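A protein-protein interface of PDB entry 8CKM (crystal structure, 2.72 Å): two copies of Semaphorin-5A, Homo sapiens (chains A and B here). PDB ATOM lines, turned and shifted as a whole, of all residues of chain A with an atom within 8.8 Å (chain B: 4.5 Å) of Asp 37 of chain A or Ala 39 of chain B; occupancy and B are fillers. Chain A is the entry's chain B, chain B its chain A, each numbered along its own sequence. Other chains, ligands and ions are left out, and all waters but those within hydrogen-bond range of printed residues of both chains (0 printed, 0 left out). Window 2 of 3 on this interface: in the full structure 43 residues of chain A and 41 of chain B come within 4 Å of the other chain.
O of Gly 40 of chain A sits close to O of Gly 40 of chain B, 2.9 Å away.
The side-chain sulfur (SG) of Cys 32 of chain A forms a disulfide with the side-chain sulfur (SG) of Cys 38 of chain A (2.0 Å).
Among the printed residues, merely in contact across the chains: Ala 39 of chain A with Asp 37 of chain B, Ala 39 of chain A with Cys 38 of chain B, Cys 38 of chain A with Ala 39 of chain B, Asp 37 of chain A with Ala 39 of chain B, Gly 40 of chain A with Cys 38 of chain B, Cys 38 of chain A with Cys 38 of chain B and Cys 41 of chain A with Gly 40 of chain B.
Asp 37 of chain A touches one residue of chain B. Of chain A, only Asp 37 and Cys 38 come within 4 Å of Ala 39 of chain B. Of chain A, only Cys 38, Ala 39 and Gly 40 come within 4 Å of Cys 38 of chain B. Of the printed residues of chain B, Gly 40 of chain A touches Cys 38 (3.7 Å) and Gly 40 (2.9 Å). Printed residues of chain A within 4 Å of Asp 37 of chain B: Ala 39 (3.3 Å). Trp 8 of chain A touches none of the printed residues of chain B. Asn 34 of chain A touches none of the printed residues of chain B. The nearest printed residue of chain B that does not touch Asp 37 of chain A is Gly 40 of chain B (5.4 Å). The nearest residue of chain A that does not touch Ala 39 of chain B is Gly 40 of chain A (4.9 Å).
Of the 13 printed residues of chain A, 5 touch a printed residue of chain B. Printed residues of chain A that touch a printed residue of chain B: Asp 37, Cys 38, Ala 39, Gly 40 and Cys 41. Hydrophobic or aromatic side chains of chain A within 4 Å of the printed part of chain B: Ala 39. Along chain A the printed residues that touch a printed residue of chain B span positions 37 to 41. Of the 6 printed residues of chain B, 4 touch a printed residue of chain A. Hydrophobic or aromatic side chains of chain B that line the printed part of chain A: Ala 39. Among the printed residues, 8 pairs touch across the chains.
Asp 37 of chain A touches Ala 39 of chain B, and with the chains exchanged Ala 39 of chain A touches Asp 37 of chain B. Cys 38 of chain A touches its own counterpart, Cys 38 of chain B. Gly 40 of chain A touches Cys 38 of chain B, but with the chains exchanged Cys 38 of chain A does not touch Gly 40 of chain B (4.03 Å). Gly 40 of chain B touches its own counterpart, Gly 40 of chain A. Positions printed for both chains: 8, 37, 38, 39 and 40. Of the 8 pairs that touch across the chains among the printed residues, 6 have their exchanged pair printed and touching as well.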
ATOM      1  N   PHE A   7      10.073  11.534   1.296  1.00  0.00           N
ATOM      2  CA  PHE A   7       9.520  11.790   2.621  1.00  0.00           C
ATOM      3  C   PHE A   7       8.701  13.078   2.634  1.00  0.00           C
ATOM      4  O   PHE A   7       9.032  14.041   1.939  1.00  0.00           O
ATOM      5  CB  PHE A   7      10.637  11.865   3.671  1.00  0.00           C
ATOM      6  CG  PHE A   7      11.601  13.003   3.461  1.00  0.00           C
ATOM      7  CD1 PHE A   7      12.671  12.871   2.592  1.00  0.00           C
ATOM      8  CD2 PHE A   7      11.446  14.200   4.144  1.00  0.00           C
ATOM      9  CE1 PHE A   7      13.559  13.912   2.399  1.00  0.00           C
ATOM     10  CE2 PHE A   7      12.332  15.246   3.955  1.00  0.00           C
ATOM     11  CZ  PHE A   7      13.391  15.100   3.082  1.00  0.00           C
ATOM     12  N   TRP A   8       7.630  13.089   3.424  1.00  0.00           N
ATOM     13  CA  TRP A   8       6.840  14.297   3.602  1.00  0.00           C
ATOM     14  C   TRP A   8       7.655  15.373   4.310  1.00  0.00           C
ATOM     15  O   TRP A   8       8.485  15.086   5.179  1.00  0.00           O
ATOM     16  CB  TRP A   8       5.576  14.007   4.414  1.00  0.00           C
ATOM     17  CG  TRP A   8       4.569  13.129   3.738  1.00  0.00           C
ATOM     18  CD1 TRP A   8       4.211  11.866   4.106  1.00  0.00           C
ATOM     19  CD2 TRP A   8       3.773  13.455   2.592  1.00  0.00           C
ATOM     20  NE1 TRP A   8       3.247  11.382   3.257  1.00  0.00           N
ATOM     21  CE2 TRP A   8       2.960  12.339   2.319  1.00  0.00           C
ATOM     22  CE3 TRP A   8       3.674  14.580   1.768  1.00  0.00           C
ATOM     23  CZ2 TRP A   8       2.059  12.315   1.256  1.00  0.00           C
ATOM     24  CZ3 TRP A   8       2.780  14.553   0.716  1.00  0.00           C
ATOM     25  CH2 TRP A   8       1.986  13.427   0.467  1.00  0.00           C
ATOM     26  N   CYS A  32       5.889  15.965  -0.954  1.00  0.00           N
ATOM     27  CA  CYS A  32       6.641  14.712  -0.995  1.00  0.00           C
ATOM     28  C   CYS A  32       7.954  14.982  -1.719  1.00  0.00           C
ATOM     29  O   CYS A  32       8.004  15.026  -2.951  1.00  0.00           O
ATOM     30  CB  CYS A  32       5.827  13.625  -1.692  1.00  0.00           C
ATOM     31  SG  CYS A  32       6.625  12.008  -1.859  1.00  0.00           S
ATOM     32  N   GLU A  33       9.026  15.160  -0.950  1.00  0.00           N
ATOM     33  CA  GLU A  33      10.321  15.513  -1.519  1.00  0.00           C
ATOM     34  C   GLU A  33      10.885  14.356  -2.331  1.00  0.00           C
ATOM     35  O   GLU A  33      10.940  13.216  -1.857  1.00  0.00           O
ATOM     36  CB  GLU A  33      11.303  15.904  -0.410  1.00  0.00           C
ATOM     37  CG  GLU A  33      11.090  17.294   0.164  1.00  0.00           C
ATOM     38  CD  GLU A  33      11.851  18.370  -0.595  1.00  0.00           C
ATOM     39  OE1 GLU A  33      12.197  18.145  -1.774  1.00  0.00           O
ATOM     40  OE2 GLU A  33      12.114  19.440  -0.006  1.00  0.00           O
ATOM     41  N   ASN A  34      11.306  14.663  -3.560  1.00  0.00           N
ATOM     42  CA  ASN A  34      11.920  13.696  -4.475  1.00  0.00           C
ATOM     43  C   ASN A  34      11.040  12.467  -4.691  1.00  0.00           C
ATOM     44  O   ASN A  34      11.540  11.347  -4.829  1.00  0.00           O
ATOM     45  CB  ASN A  34      13.310  13.275  -3.990  1.00  0.00           C
ATOM     46  N   GLY A  35       9.725  12.663  -4.728  1.00  0.00           N
ATOM     47  CA  GLY A  35       8.803  11.567  -4.897  1.00  0.00           C
ATOM     48  C   GLY A  35       7.432  12.018  -5.351  1.00  0.00           C
ATOM     49  O   GLY A  35       6.905  13.039  -4.898  1.00  0.00           O
ATOM     50  N   PRO A  36       6.829  11.265  -6.271  1.00  0.00           N
ATOM     51  CA  PRO A  36       5.479  11.605  -6.736  1.00  0.00           C
ATOM     52  C   PRO A  36       4.397  11.028  -5.839  1.00  0.00           C
ATOM     53  O   PRO A  36       3.322  11.615  -5.686  1.00  0.00           O
ATOM     54  CB  PRO A  36       5.435  10.989  -8.138  1.00  0.00           C
ATOM     55  CG  PRO A  36       6.332   9.797  -8.033  1.00  0.00           C
ATOM     56  CD  PRO A  36       7.419  10.156  -7.043  1.00  0.00           C
ATOM     57  N   ASP A  37       4.677   9.874  -5.238  1.00  0.00           N
ATOM     58  CA  ASP A  37       3.707   9.147  -4.424  1.00  0.00           C
ATOM     59  C   ASP A  37       4.352   8.779  -3.092  1.00  0.00           C
ATOM     60  O   ASP A  37       5.022   7.746  -2.981  1.00  0.00           O
ATOM     61  CB  ASP A  37       3.206   7.905  -5.153  1.00  0.00           C
ATOM     62  N   CYS A  38       4.155   9.631  -2.089  1.00  0.00           N
ATOM     63  CA  CYS A  38       4.474   9.286  -0.715  1.00  0.00           C
ATOM     64  C   CYS A  38       3.308   8.517  -0.092  1.00  0.00           C
ATOM     65  O   CYS A  38       2.229   8.386  -0.672  1.00  0.00           O
ATOM     66  CB  CYS A  38       4.796  10.538   0.107  1.00  0.00           C
ATOM     67  SG  CYS A  38       6.501  11.175  -0.009  1.00  0.00           S
ATOM     68  N   ALA A  39       3.537   8.017   1.122  1.00  0.00           N
ATOM     69  CA  ALA A  39       2.611   7.116   1.794  1.00  0.00           C
ATOM     70  C   ALA A  39       1.513   7.847   2.556  1.00  0.00           C
ATOM     71  O   ALA A  39       1.087   7.384   3.621  1.00  0.00           O
ATOM     72  CB  ALA A  39       3.384   6.197   2.735  1.00  0.00           C
ATOM     73  N   GLY A  40       1.023   8.963   2.032  1.00  0.00           N
ATOM     74  CA  GLY A  40      -0.016   9.696   2.716  1.00  0.00           C
ATOM     75  C   GLY A  40      -0.742  10.647   1.798  1.00  0.00           C
ATOM     76  O   GLY A  40      -0.600  10.591   0.574  1.00  0.00           O
ATOM     77  N   CYS A  41      -1.520  11.532   2.412  1.00  0.00           N
ATOM     78  CA  CYS A  41      -2.282  12.539   1.693  1.00  0.00           C
ATOM     79  C   CYS A  41      -1.613  13.891   1.885  1.00  0.00           C
ATOM     80  O   CYS A  41      -1.272  14.263   3.012  1.00  0.00           O
ATOM     81  CB  CYS A  41      -3.727  12.569   2.180  1.00  0.00           C
ATOM     82  SG  CYS A  41      -4.718  13.811   1.386  1.00  0.00           S
ATOM     83  N   ASN A  42      -1.397  14.610   0.781  1.00  0.00           N
ATOM     84  CA  ASN A  42      -0.596  15.829   0.831  1.00  0.00           C
ATOM     85  C   ASN A  42      -1.330  16.999   1.475  1.00  0.00           C
ATOM     86  O   ASN A  42      -0.672  17.904   1.998  1.00  0.00           O
ATOM     87  CB  ASN A  42      -0.124  16.222  -0.577  1.00  0.00           C
ATOM     88  CG  ASN A  42      -1.268  16.323  -1.577  1.00  0.00           C
ATOM     89  OD1 ASN A  42      -2.371  16.772  -1.248  1.00  0.00           O
ATOM     90  ND2 ASN A  42      -1.002  15.922  -2.812  1.00  0.00           N
ATOM     91  N   TRP B   8      -5.802   1.491  -4.366  1.00  0.00           N
ATOM     92  CA  TRP B   8      -7.014   2.297  -4.257  1.00  0.00           C
ATOM     93  C   TRP B   8      -8.160   1.719  -5.073  1.00  0.00           C
ATOM     94  O   TRP B   8      -7.951   1.178  -6.159  1.00  0.00           O
ATOM     95  CB  TRP B   8      -6.745   3.730  -4.710  1.00  0.00           C
ATOM     96  CG  TRP B   8      -5.823   4.462  -3.813  1.00  0.00           C
ATOM     97  CD1 TRP B   8      -4.515   4.758  -4.049  1.00  0.00           C
ATOM     98  CD2 TRP B   8      -6.130   4.994  -2.522  1.00  0.00           C
ATOM     99  NE1 TRP B   8      -3.987   5.445  -2.985  1.00  0.00           N
ATOM    100  CE2 TRP B   8      -4.959   5.603  -2.032  1.00  0.00           C
ATOM    101  CE3 TRP B   8      -7.283   5.015  -1.731  1.00  0.00           C
ATOM    102  CZ2 TRP B   8      -4.907   6.227  -0.787  1.00  0.00           C
ATOM    103  CZ3 TRP B   8      -7.229   5.632  -0.497  1.00  0.00           C
ATOM    104  CH2 TRP B   8      -6.051   6.231  -0.037  1.00  0.00           C
ATOM    105  N   ARG B  30     -12.710   7.375  -1.454  1.00  0.00           N
ATOM    106  CA  ARG B  30     -12.360   6.019  -1.847  1.00  0.00           C
ATOM    107  C   ARG B  30     -11.630   5.356  -0.687  1.00  0.00           C
ATOM    108  O   ARG B  30     -11.195   6.019   0.259  1.00  0.00           O
ATOM    109  CB  ARG B  30     -11.501   6.003  -3.117  1.00  0.00           C
ATOM    110  CG  ARG B  30     -10.158   6.693  -2.958  1.00  0.00           C
ATOM    111  CD  ARG B  30      -9.314   6.588  -4.218  1.00  0.00           C
ATOM    112  NE  ARG B  30      -8.003   7.202  -4.036  1.00  0.00           N
ATOM    113  CZ  ARG B  30      -7.061   7.252  -4.968  1.00  0.00           C
ATOM    114  NH1 ARG B  30      -7.251   6.735  -6.171  1.00  0.00           N
ATOM    115  NH2 ARG B  30      -5.900   7.834  -4.685  1.00  0.00           N
ATOM    116  N   ASP B  37      -0.947   2.579   4.550  1.00  0.00           N
ATOM    117  CA  ASP B  37      -0.450   3.837   3.996  1.00  0.00           C
ATOM    118  C   ASP B  37      -0.303   3.661   2.487  1.00  0.00           C
ATOM    119  O   ASP B  37       0.713   3.149   2.008  1.00  0.00           O
ATOM    120  CB  ASP B  37       0.874   4.240   4.645  1.00  0.00           C
ATOM    121  CG  ASP B  37       0.764   4.398   6.149  1.00  0.00           C
ATOM    122  OD1 ASP B  37      -0.324   4.771   6.634  1.00  0.00           O
ATOM    123  OD2 ASP B  37       1.764   4.150   6.853  1.00  0.00           O
ATOM    124  N   CYS B  38      -1.311   4.097   1.738  1.00  0.00           N
ATOM    125  CA  CYS B  38      -1.316   3.970   0.290  1.00  0.00           C
ATOM    126  C   CYS B  38      -0.937   5.291  -0.369  1.00  0.00           C
ATOM    127  O   CYS B  38      -0.840   6.338   0.273  1.00  0.00           O
ATOM    128  CB  CYS B  38      -2.685   3.496  -0.199  1.00  0.00           C
ATOM    129  SG  CYS B  38      -3.222   1.948   0.549  1.00  0.00           S
ATOM    130  N   ALA B  39      -0.721   5.224  -1.678  1.00  0.00           N
ATOM    131  CA  ALA B  39      -0.228   6.357  -2.450  1.00  0.00           C
ATOM    132  C   ALA B  39      -1.397   7.237  -2.873  1.00  0.00           C
ATOM    133  O   ALA B  39      -2.250   6.810  -3.659  1.00  0.00           O
ATOM    134  CB  ALA B  39       0.547   5.871  -3.674  1.00  0.00           C
ATOM    135  N   GLY B  40      -1.427   8.460  -2.368  1.00  0.00           N
ATOM    136  CA  GLY B  40      -2.438   9.429  -2.738  1.00  0.00           C
ATOM    137  C   GLY B  40      -3.347   9.781  -1.574  1.00  0.00           C
ATOM    138  O   GLY B  40      -3.102   9.433  -0.416  1.00  0.00           O
